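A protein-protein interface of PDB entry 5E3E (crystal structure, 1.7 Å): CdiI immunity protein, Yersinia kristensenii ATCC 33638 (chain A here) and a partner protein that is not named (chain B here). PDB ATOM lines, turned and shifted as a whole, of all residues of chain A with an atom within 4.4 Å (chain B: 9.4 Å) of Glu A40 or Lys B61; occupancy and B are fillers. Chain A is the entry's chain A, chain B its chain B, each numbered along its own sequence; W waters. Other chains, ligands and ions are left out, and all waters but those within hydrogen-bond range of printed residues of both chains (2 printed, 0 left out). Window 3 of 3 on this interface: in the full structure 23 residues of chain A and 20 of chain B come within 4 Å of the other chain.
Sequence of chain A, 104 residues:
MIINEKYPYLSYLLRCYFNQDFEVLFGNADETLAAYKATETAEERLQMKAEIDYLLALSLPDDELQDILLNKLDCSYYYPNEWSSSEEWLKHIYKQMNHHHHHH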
ATOM      1  N   TYR A  12      -9.788  -8.870   6.737  1.00  0.00           N
ATOM      2  CA  TYR A  12     -10.483  -9.330   7.930  1.00  0.00           C
ATOM      3  C   TYR A  12     -10.847 -10.817   7.823  1.00  0.00           C
ATOM      4  O   TYR A  12     -10.518 -11.580   8.738  1.00  0.00           O
ATOM      5  CB  TYR A  12     -11.738  -8.493   8.182  1.00  0.00           C
ATOM      6  CG  TYR A  12     -12.552  -8.941   9.364  1.00  0.00           C
ATOM      7  CD1 TYR A  12     -12.067  -8.802  10.662  1.00  0.00           C
ATOM      8  CD2 TYR A  12     -13.770  -9.527   9.189  1.00  0.00           C
ATOM      9  CE1 TYR A  12     -12.809  -9.213  11.761  1.00  0.00           C
ATOM     10  CE2 TYR A  12     -14.509  -9.963  10.272  1.00  0.00           C
ATOM     11  CZ  TYR A  12     -14.050  -9.794  11.561  1.00  0.00           C
ATOM     12  OH  TYR A  12     -14.817 -10.212  12.663  1.00  0.00           O
ATOM     13  N   TYR A  17     -10.465 -14.877  10.359  1.00  0.00           N
ATOM     14  CA  TYR A  17     -11.144 -16.144  10.231  1.00  0.00           C
ATOM     15  C   TYR A  17     -10.164 -17.196   9.756  1.00  0.00           C
ATOM     16  O   TYR A  17     -10.042 -18.221  10.426  1.00  0.00           O
ATOM     17  CB  TYR A  17     -12.389 -16.059   9.319  1.00  0.00           C
ATOM     18  CG  TYR A  17     -13.568 -15.483  10.077  1.00  0.00           C
ATOM     19  CD1 TYR A  17     -13.721 -14.117  10.246  1.00  0.00           C
ATOM     20  CD2 TYR A  17     -14.510 -16.349  10.685  1.00  0.00           C
ATOM     21  CE1 TYR A  17     -14.771 -13.613  10.989  1.00  0.00           C
ATOM     22  CE2 TYR A  17     -15.575 -15.857  11.386  1.00  0.00           C
ATOM     23  CZ  TYR A  17     -15.708 -14.492  11.540  1.00  0.00           C
ATOM     24  OH  TYR A  17     -16.766 -14.005  12.274  1.00  0.00           O
ATOM     25  N   TYR A  36     -18.167 -17.184   9.499  1.00  0.00           N
ATOM     26  CA  TYR A  36     -18.110 -15.786   9.113  1.00  0.00           C
ATOM     27  C   TYR A  36     -19.501 -15.285   8.702  1.00  0.00           C
ATOM     28  O   TYR A  36     -19.969 -14.242   9.164  1.00  0.00           O
ATOM     29  CB  TYR A  36     -17.108 -15.644   7.992  1.00  0.00           C
ATOM     30  CG  TYR A  36     -17.121 -14.336   7.282  1.00  0.00           C
ATOM     31  CD1 TYR A  36     -16.284 -13.303   7.685  1.00  0.00           C
ATOM     32  CD2 TYR A  36     -17.874 -14.150   6.148  1.00  0.00           C
ATOM     33  CE1 TYR A  36     -16.258 -12.089   7.019  1.00  0.00           C
ATOM     34  CE2 TYR A  36     -17.845 -12.940   5.458  1.00  0.00           C
ATOM     35  CZ  TYR A  36     -17.047 -11.915   5.891  1.00  0.00           C
ATOM     36  OH  TYR A  36     -17.023 -10.748   5.181  1.00  0.00           O
ATOM     37  N   LYS A  37     -20.159 -16.039   7.861  1.00  0.00           N
ATOM     38  CA  LYS A  37     -21.459 -15.633   7.371  1.00  0.00           C
ATOM     39  C   LYS A  37     -22.430 -15.485   8.532  1.00  0.00           C
ATOM     40  O   LYS A  37     -23.221 -14.520   8.554  1.00  0.00           O
ATOM     41  CB  LYS A  37     -22.009 -16.617   6.336  1.00  0.00           C
ATOM     42  CG  LYS A  37     -23.383 -16.161   5.814  1.00  0.00           C
ATOM     43  CD  LYS A  37     -23.882 -16.979   4.657  1.00  0.00           C
ATOM     44  CE  LYS A  37     -25.256 -16.453   4.293  1.00  0.00           C
ATOM     45  NZ  LYS A  37     -25.903 -17.197   3.193  1.00  0.00           N
ATOM     46  N   ALA A  38     -22.407 -16.434   9.468  1.00  0.00           N
ATOM     47  CA  ALA A  38     -23.342 -16.417  10.588  1.00  0.00           C
ATOM     48  C   ALA A  38     -23.074 -15.284  11.566  1.00  0.00           C
ATOM     49  O   ALA A  38     -24.014 -14.719  12.152  1.00  0.00           O
ATOM     50  CB  ALA A  38     -23.314 -17.741  11.328  1.00  0.00           C
ATOM     51  N   THR A  39     -21.808 -14.967  11.755  1.00  0.00           N
ATOM     52  CA  THR A  39     -21.372 -14.039  12.780  1.00  0.00           C
ATOM     53  C   THR A  39     -21.440 -12.586  12.318  1.00  0.00           C
ATOM     54  O   THR A  39     -21.901 -11.708  13.081  1.00  0.00           O
ATOM     55  CB  THR A  39     -19.920 -14.385  13.214  1.00  0.00           C
ATOM     56  OG1 THR A  39     -19.877 -15.726  13.709  1.00  0.00           O
ATOM     57  CG2 THR A  39     -19.447 -13.446  14.310  1.00  0.00           C
ATOM     58  N   GLU A  40     -21.027 -12.324  11.075  1.00  0.00           N
ATOM     59  CA  GLU A  40     -20.857 -10.964  10.589  1.00  0.00           C
ATOM     60  C   GLU A  40     -22.130 -10.450   9.914  1.00  0.00           C
ATOM     61  O   GLU A  40     -23.034 -11.232   9.569  1.00  0.00           O
ATOM     62  CB  GLU A  40     -19.679 -10.862   9.635  1.00  0.00           C
ATOM     63  CG  GLU A  40     -18.358 -11.425  10.177  1.00  0.00           C
ATOM     64  CD  GLU A  40     -17.854 -10.757  11.455  1.00  0.00           C
ATOM     65  OE1 GLU A  40     -18.205  -9.589  11.693  1.00  0.00           O
ATOM     66  OE2 GLU A  40     -17.015 -11.338  12.197  1.00  0.00           O
ATOM     67  N   THR A  41     -22.237  -9.134   9.772  1.00  0.00           N
ATOM     68  CA  THR A  41     -23.456  -8.540   9.208  1.00  0.00           C
ATOM     69  C   THR A  41     -23.518  -8.751   7.707  1.00  0.00           C
ATOM     70  O   THR A  41     -22.502  -9.068   7.060  1.00  0.00           O
ATOM     71  CB  THR A  41     -23.498  -7.041   9.466  1.00  0.00           C
ATOM     72  OG1 THR A  41     -22.435  -6.406   8.750  1.00  0.00           O
ATOM     73  CG2 THR A  41     -23.350  -6.765  10.961  1.00  0.00           C
ATOM     74  N   ALA A  42     -24.700  -8.546   7.149  1.00  0.00           N
ATOM     75  CA  ALA A  42     -24.865  -8.600   5.697  1.00  0.00           C
ATOM     76  C   ALA A  42     -23.985  -7.516   5.040  1.00  0.00           C
ATOM     77  O   ALA A  42     -23.383  -7.762   3.982  1.00  0.00           O
ATOM     78  CB  ALA A  42     -26.337  -8.382   5.320  1.00  0.00           C
ATOM     79  N   GLU A  44     -21.098  -6.387   6.061  1.00  0.00           N
ATOM     80  CA  GLU A  44     -19.732  -6.833   6.072  1.00  0.00           C
ATOM     81  C   GLU A  44     -19.475  -7.788   4.905  1.00  0.00           C
ATOM     82  O   GLU A  44     -18.491  -7.625   4.159  1.00  0.00           O
ATOM     83  CB  GLU A  44     -19.380  -7.472   7.415  1.00  0.00           C
ATOM     84  CG  GLU A  44     -17.953  -7.944   7.534  1.00  0.00           C
ATOM     85  CD  GLU A  44     -16.961  -6.834   7.836  1.00  0.00           C
ATOM     86  OE1 GLU A  44     -15.737  -7.108   7.780  1.00  0.00           O
ATOM     87  OE2 GLU A  44     -17.355  -5.688   8.159  1.00  0.00           O
ATOM     88  N   LYS B  51      -7.906   1.805  19.036  1.00  0.00           N
ATOM     89  CA  LYS B  51      -8.567   0.874  18.123  1.00  0.00           C
ATOM     90  C   LYS B  51      -9.488  -0.150  18.860  1.00  0.00           C
ATOM     91  O   LYS B  51     -10.595  -0.456  18.398  1.00  0.00           O
ATOM     92  CB  LYS B  51      -7.470   0.156  17.344  1.00  0.00           C
ATOM     93  CG  LYS B  51      -7.876  -0.631  16.137  1.00  0.00           C
ATOM     94  CD  LYS B  51      -6.642  -1.244  15.505  1.00  0.00           C
ATOM     95  CE  LYS B  51      -7.021  -2.253  14.445  1.00  0.00           C
ATOM     96  NZ  LYS B  51      -5.789  -2.846  13.846  1.00  0.00           N
ATOM     97  N   ILE B  52      -9.039  -0.671  19.997  1.00  0.00           N
ATOM     98  CA  ILE B  52      -9.854  -1.593  20.787  1.00  0.00           C
ATOM     99  C   ILE B  52     -11.092  -0.860  21.347  1.00  0.00           C
ATOM    100  O   ILE B  52     -12.213  -1.400  21.354  1.00  0.00           O
ATOM    101  CB  ILE B  52      -9.054  -2.195  21.958  1.00  0.00           C
ATOM    102  CG1 ILE B  52      -7.953  -3.127  21.430  1.00  0.00           C
ATOM    103  CG2 ILE B  52      -9.963  -2.962  22.908  1.00  0.00           C
ATOM    104  CD1 ILE B  52      -6.885  -3.446  22.460  1.00  0.00           C
ATOM    105  N   SER B  54     -12.629   1.879  20.226  1.00  0.00           N
ATOM    106  CA  SER B  54     -13.601   2.118  19.141  1.00  0.00           C
ATOM    107  C   SER B  54     -14.328   0.850  18.751  1.00  0.00           C
ATOM    108  O   SER B  54     -15.523   0.884  18.485  1.00  0.00           O
ATOM    109  CB  SER B  54     -12.914   2.665  17.887  1.00  0.00           C
ATOM    110  OG  SER B  54     -12.205   3.852  18.193  1.00  0.00           O
ATOM    111  N   TYR B  55     -13.581  -0.259  18.684  1.00  0.00           N
ATOM    112  CA  TYR B  55     -14.153  -1.550  18.319  1.00  0.00           C
ATOM    113  C   TYR B  55     -15.249  -1.948  19.316  1.00  0.00           C
ATOM    114  O   TYR B  55     -16.342  -2.322  18.902  1.00  0.00           O
ATOM    115  CB  TYR B  55     -13.062  -2.630  18.196  1.00  0.00           C
ATOM    116  CG  TYR B  55     -13.573  -4.060  18.230  1.00  0.00           C
ATOM    117  CD1 TYR B  55     -14.118  -4.662  17.084  1.00  0.00           C
ATOM    118  CD2 TYR B  55     -13.517  -4.810  19.390  1.00  0.00           C
ATOM    119  CE1 TYR B  55     -14.571  -5.960  17.113  1.00  0.00           C
ATOM    120  CE2 TYR B  55     -13.974  -6.114  19.421  1.00  0.00           C
ATOM    121  CZ  TYR B  55     -14.502  -6.678  18.264  1.00  0.00           C
ATOM    122  OH  TYR B  55     -14.983  -7.967  18.269  1.00  0.00           O
ATOM    123  N   LEU B  56     -14.998  -1.805  20.609  1.00  0.00           N
ATOM    124  CA  LEU B  56     -15.949  -2.256  21.637  1.00  0.00           C
ATOM    125  C   LEU B  56     -17.219  -1.387  21.698  1.00  0.00           C
ATOM    126  O   LEU B  56     -18.320  -1.884  21.926  1.00  0.00           O
ATOM    127  CB  LEU B  56     -15.288  -2.262  23.019  1.00  0.00           C
ATOM    128  CG  LEU B  56     -14.167  -3.281  23.194  1.00  0.00           C
ATOM    129  CD1 LEU B  56     -13.458  -3.039  24.520  1.00  0.00           C
ATOM    130  CD2 LEU B  56     -14.684  -4.705  23.095  1.00  0.00           C
ATOM    131  N   SER B  57     -17.057  -0.101  21.460  1.00  0.00           N
ATOM    132  CA  SER B  57     -18.173   0.839  21.622  1.00  0.00           C
ATOM    133  C   SER B  57     -19.028   0.952  20.361  1.00  0.00           C
ATOM    134  O   SER B  57     -20.235   1.197  20.432  1.00  0.00           O
ATOM    135  CB  SER B  57     -17.625   2.214  22.022  1.00  0.00           C
ATOM    136  OG  SER B  57     -16.969   2.832  20.925  1.00  0.00           O
ATOM    137  N   GLY B  58     -18.409   0.799  19.200  1.00  0.00           N
ATOM    138  CA  GLY B  58     -19.100   1.077  17.948  1.00  0.00           C
ATOM    139  C   GLY B  58     -19.283  -0.040  16.935  1.00  0.00           C
ATOM    140  O   GLY B  58     -20.058   0.129  16.002  1.00  0.00           O
ATOM    141  N   SER B  59     -18.585  -1.162  17.089  1.00  0.00           N
ATOM    142  CA  SER B  59     -18.521  -2.170  16.021  1.00  0.00           C
ATOM    143  C   SER B  59     -19.365  -3.418  16.273  1.00  0.00           C
ATOM    144  O   SER B  59     -19.409  -3.930  17.397  1.00  0.00           O
ATOM    145  CB  SER B  59     -17.073  -2.629  15.812  1.00  0.00           C
ATOM    146  OG  SER B  59     -16.972  -3.340  14.596  1.00  0.00           O
ATOM    147  N   GLN B  60     -19.959  -3.949  15.219  1.00  0.00           N
ATOM    148  CA  GLN B  60     -20.627  -5.246  15.292  1.00  0.00           C
ATOM    149  C   GLN B  60     -19.708  -6.422  14.839  1.00  0.00           C
ATOM    150  O   GLN B  60     -20.137  -7.561  14.801  1.00  0.00           O
ATOM    151  CB  GLN B  60     -21.933  -5.191  14.496  1.00  0.00           C
ATOM    152  CG  GLN B  60     -22.893  -4.161  15.097  1.00  0.00           C
ATOM    153  CD  GLN B  60     -24.251  -4.078  14.421  1.00  0.00           C
ATOM    154  OE1 GLN B  60     -24.781  -2.976  14.183  1.00  0.00           O
ATOM    155  NE2 GLN B  60     -24.863  -5.228  14.179  1.00  0.00           N
ATOM    156  N   LYS B  61     -18.442  -6.134  14.550  1.00  0.00           N
ATOM    157  CA  LYS B  61     -17.510  -7.175  14.124  1.00  0.00           C
ATOM    158  C   LYS B  61     -17.322  -8.278  15.174  1.00  0.00           C
ATOM    159  O   LYS B  61     -17.276  -8.005  16.383  1.00  0.00           O
ATOM    160  CB  LYS B  61     -16.149  -6.560  13.799  1.00  0.00           C
ATOM    161  CG  LYS B  61     -16.096  -5.793  12.488  1.00  0.00           C
ATOM    162  CD  LYS B  61     -14.718  -5.182  12.337  1.00  0.00           C
ATOM    163  CE  LYS B  61     -13.672  -6.294  12.337  1.00  0.00           C
ATOM    164  NZ  LYS B  61     -12.484  -6.018  13.186  1.00  0.00           N
ATOM    165  N   GLY B  62     -17.202  -9.523  14.712  1.00  0.00           N
ATOM    166  CA  GLY B  62     -16.994 -10.645  15.620  1.00  0.00           C
ATOM    167  C   GLY B  62     -15.630 -10.644  16.281  1.00  0.00           C
ATOM    168  O   GLY B  62     -15.486 -11.113  17.431  1.00  0.00           O
ATOM    169  N   TYR B  63     -14.631 -10.154  15.556  1.00  0.00           N
ATOM    170  CA  TYR B  63     -13.225 -10.180  16.007  1.00  0.00           C
ATOM    171  C   TYR B  63     -12.552  -8.864  15.692  1.00  0.00           C
ATOM    172  O   TYR B  63     -13.057  -8.086  14.881  1.00  0.00           O
ATOM    173  CB  TYR B  63     -12.459 -11.333  15.314  1.00  0.00           C
ATOM    174  CG  TYR B  63     -13.129 -12.662  15.551  1.00  0.00           C
ATOM    175  CD1 TYR B  63     -14.161 -13.107  14.719  1.00  0.00           C
ATOM    176  CD2 TYR B  63     -12.834 -13.412  16.685  1.00  0.00           C
ATOM    177  CE1 TYR B  63     -14.826 -14.304  14.961  1.00  0.00           C
ATOM    178  CE2 TYR B  63     -13.485 -14.609  16.944  1.00  0.00           C
ATOM    179  CZ  TYR B  63     -14.476 -15.063  16.093  1.00  0.00           C
ATOM    180  OH  TYR B  63     -15.177 -16.247  16.328  1.00  0.00           O
ATOM    181  N   LEU B  64     -11.381  -8.666  16.271  1.00  0.00           N
ATOM    182  CA  LEU B  64     -10.504  -7.539  15.950  1.00  0.00           C
ATOM    183  C   LEU B  64      -9.046  -8.019  15.890  1.00  0.00           C
ATOM    184  O   LEU B  64      -8.560  -8.704  16.784  1.00  0.00           O
ATOM    185  CB  LEU B  64     -10.632  -6.425  16.983  1.00  0.00           C
ATOM    186  CG  LEU B  64      -9.753  -5.167  16.756  1.00  0.00           C
ATOM    187  CD1 LEU B  64     -10.261  -4.307  15.606  1.00  0.00           C
ATOM    188  CD2 LEU B  64      -9.676  -4.359  18.028  1.00  0.00           C
ATOM    189  N   GLU B  65      -8.381  -7.630  14.816  1.00  0.00           N
ATOM    190  CA  GLU B  65      -6.945  -7.862  14.606  1.00  0.00           C
ATOM    191  C   GLU B  65      -6.148  -6.718  15.201  1.00  0.00           C
ATOM    192  O   GLU B  65      -6.428  -5.551  14.905  1.00  0.00           O
ATOM    193  CB  GLU B  65      -6.683  -7.888  13.089  1.00  0.00           C
ATOM    194  CG  GLU B  65      -5.217  -7.915  12.675  1.00  0.00           C
ATOM    195  CD  GLU B  65      -5.016  -7.782  11.175  1.00  0.00           C
ATOM    196  OE1 GLU B  65      -6.004  -7.937  10.388  1.00  0.00           O
ATOM    197  OE2 GLU B  65      -3.824  -7.560  10.783  1.00  0.00           O
ATOM    198  N   ILE B  66      -5.132  -7.024  16.010  1.00  0.00           N
ATOM    199  CA  ILE B  66      -4.236  -6.006  16.468  1.00  0.00           C
ATOM    200  C   ILE B  66      -2.836  -6.496  16.197  1.00  0.00           C
ATOM    201  O   ILE B  66      -2.495  -7.626  16.520  1.00  0.00           O
ATOM    202  CB  ILE B  66      -4.420  -5.623  17.945  1.00  0.00           C
ATOM    203  CG1 ILE B  66      -4.205  -6.800  18.859  1.00  0.00           C
ATOM    204  CG2 ILE B  66      -5.832  -5.053  18.168  1.00  0.00           C
ATOM    205  CD1 ILE B  66      -3.945  -6.430  20.305  1.00  0.00           C
ATOM    206  N   ILE B  93      -2.347 -10.417  17.132  1.00  0.00           N
ATOM    207  CA  ILE B  93      -3.239 -10.934  18.149  1.00  0.00           C
ATOM    208  C   ILE B  93      -4.658 -10.809  17.640  1.00  0.00           C
ATOM    209  O   ILE B  93      -4.988  -9.813  17.015  1.00  0.00           O
ATOM    210  CB  ILE B  93      -3.125 -10.094  19.465  1.00  0.00           C
ATOM    211  CG1 ILE B  93      -1.654  -9.919  19.921  1.00  0.00           C
ATOM    212  CG2 ILE B  93      -3.998 -10.681  20.551  1.00  0.00           C
ATOM    213  CD1 ILE B  93      -0.852 -11.131  20.086  1.00  0.00           C
ATOM    214  N   ILE B  94      -5.502 -11.799  17.896  1.00  0.00           N
ATOM    215  CA  ILE B  94      -6.909 -11.699  17.515  1.00  0.00           C
ATOM    216  C   ILE B  94      -7.722 -11.702  18.784  1.00  0.00           C
ATOM    217  O   ILE B  94      -7.579 -12.634  19.597  1.00  0.00           O
ATOM    218  CB  ILE B  94      -7.376 -12.884  16.632  1.00  0.00           C
ATOM    219  CG1 ILE B  94      -6.552 -13.010  15.338  1.00  0.00           C
ATOM    220  CG2 ILE B  94      -8.873 -12.771  16.290  1.00  0.00           C
ATOM    221  CD1 ILE B  94      -6.457 -11.753  14.546  1.00  0.00           C
ATOM    222  N   ILE B  95      -8.583 -10.702  18.945  1.00  0.00           N
ATOM    223  CA  ILE B  95      -9.482 -10.626  20.093  1.00  0.00           C
ATOM    224  C   ILE B  95     -10.932 -10.698  19.659  1.00  0.00           C
ATOM    225  O   ILE B  95     -11.258 -10.513  18.491  1.00  0.00           O
ATOM    226  CB  ILE B  95      -9.228  -9.377  20.952  1.00  0.00           C
ATOM    227  CG1 ILE B  95      -9.622  -8.081  20.224  1.00  0.00           C
ATOM    228  CG2 ILE B  95      -7.787  -9.341  21.382  1.00  0.00           C
ATOM    229  CD1 ILE B  95      -9.629  -6.860  21.125  1.00  0.00           C
ATOM    230  N   ALA B  96     -11.787 -11.028  20.603  1.00  0.00           N
ATOM    231  CA  ALA B  96     -13.210 -11.037  20.333  1.00  0.00           C
ATOM    232  C   ALA B  96     -13.953 -10.343  21.440  1.00  0.00           C
ATOM    233  O   ALA B  96     -13.580 -10.437  22.605  1.00  0.00           O
ATOM    234  CB  ALA B  96     -13.710 -12.450  20.192  1.00  0.00           C
ATOM    235  N   ARG B  97     -15.030  -9.652  21.079  1.00  0.00           N
ATOM    236  CA  ARG B  97     -15.824  -8.932  22.053  1.00  0.00           C
ATOM    237  C   ARG B  97     -16.441  -9.967  23.000  1.00  0.00           C
ATOM    238  O   ARG B  97     -17.031 -10.945  22.541  1.00  0.00           O
ATOM    239  CB  ARG B  97     -16.906  -8.122  21.334  1.00  0.00           C
ATOM    240  CG  ARG B  97     -17.555  -7.034  22.182  1.00  0.00           C
ATOM    241  CD  ARG B  97     -18.633  -6.290  21.410  1.00  0.00           C
ATOM    242  NE  ARG B  97     -18.129  -5.702  20.169  1.00  0.00           N
ATOM    243  CZ  ARG B  97     -18.206  -6.289  18.973  1.00  0.00           C
ATOM    244  NH1 ARG B  97     -17.715  -5.681  17.911  1.00  0.00           N
ATOM    245  NH2 ARG B  97     -18.796  -7.461  18.839  1.00  0.00           N
ATOM    246  N   ASP B  98     -16.282  -9.746  24.305  1.00  0.00           N
ATOM    247  CA  ASP B  98     -16.751 -10.667  25.348  1.00  0.00           C
ATOM    248  C   ASP B  98     -17.131  -9.858  26.592  1.00  0.00           C
ATOM    249  O   ASP B  98     -16.320  -9.705  27.516  1.00  0.00           O
ATOM    250  CB  ASP B  98     -15.667 -11.693  25.697  1.00  0.00           C
ATOM    251  CG  ASP B  98     -16.172 -12.779  26.650  1.00  0.00           C
ATOM    252  OD1 ASP B  98     -17.347 -12.708  27.045  1.00  0.00           O
ATOM    253  OD2 ASP B  98     -15.398 -13.700  27.003  1.00  0.00           O
ATOM    254  N   GLY B 104     -13.647  -6.313  28.483  1.00  0.00           N
ATOM    255  CA  GLY B 104     -14.696  -6.368  27.464  1.00  0.00           C
ATOM    256  C   GLY B 104     -14.386  -7.285  26.283  1.00  0.00           C
ATOM    257  O   GLY B 104     -15.179  -7.385  25.362  1.00  0.00           O
HETATM  258  O   HOH W   1     -22.098  -8.890  13.531  1.00  0.00           O
HETATM  259  O   HOH W   2     -17.538 -16.645  15.205  1.00  0.00           O
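Printed residues of chain B within 4 Å of Tyr A12: Lys B61, Gly B62 and Tyr B63.
Printed residues of chain B within 4 Å of Glu A40: Lys B61 (3.5 Å) and Gly B62 (3.1 Å).
Thr A41 touches just one residue of chain B: Gln B60.
Gly B58 touches none of the printed residues of chain A.
Of the printed residues of chain A, Tyr B63 touches Tyr A12 and Tyr A17.
The nearest printed residue of chain B that does not touch Glu A40 is Gln B60 (4.2 Å).
The nearest printed residue of chain A that does not touch Lys B61 is Glu A44 (4.5 Å).
Of the 10 printed residues of chain A, 5 touch a printed residue of chain B.
Printed residues of chain A that touch a printed residue of chain B: Tyr A12, Tyr A17, Thr A39, Glu A40 and Thr A41.
Hydrophobic or aromatic side chains of chain A that line the printed part of chain B: Tyr A12 and Tyr A17.
Hydrophobic or aromatic side chains of chain B within 4 Å of the printed part of chain A: Tyr B63.
Among the printed residues, 8 pairs touch across the chains.
Among the printed residues, no Asp or Glu carboxylate lies within 4 Å of a Lys or Arg side-chain nitrogen of the other chain.
The guanidinium group of Arg B97 is in hydrogen-bond range of the backbone carbonyl oxygen of Lys B61, 2.8 Å away.
The backbone NH (N) of Lys B61 sits at hydrogen-bond distance from the side-chain hydroxyl (OG) of Ser B59, at 3.2 Å.
The backbone carbonyl oxygen (O) of Tyr B63 is in hydrogen-bond range of the side-chain amino group (NZ) of Lys B61 (2.7 Å).
The side-chain hydroxyl (OH) of Tyr B55 is in hydrogen-bond range of the backbone carbonyl oxygen (O) of Lys B61 (3.0 Å).
The backbone NH (N) of Glu A44 is in hydrogen-bond range of the side-chain hydroxyl (OG1) of Thr A41 (3.0 Å).
The backbone carbonyl oxygen (O) of Gly B62 lies within hydrogen-bond range of the side-chain hydroxyl (OH) of Tyr B55.
Water W2 bridges OH of Tyr B63 (2.6 Å) and OG1 of Thr A39 (2.9 Å).
Water W1 bridges the backbone carbonyl oxygen of Gln B60 and the backbone carbonyl oxygen of Thr A39.
Tyr A12 touches Lys B61 (CE1 to CE, 3.1 Å).
Tyr A17 touches Tyr B63 (OH to CE1, 3.3 Å).
CG2 of Thr A39 touches CA of Gly B62 (3.9 Å).
Glu A40 touches Lys B61.
CG2 of Thr A41 touches NE2 of Gln B60, at 3.9 Å.
N of Gly B62 sits at hydrogen-bond distance from OE2 of Glu A40 (3.1 Å).
The side-chain hydroxyl of Tyr A12 is in hydrogen-bond range of the backbone NH of Tyr B63 (2.9 Å).
The side-chain hydroxyl (OH) of Tyr A12 lies within hydrogen-bond range of the backbone NH (N) of Gly B62, 3.2 Å away.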
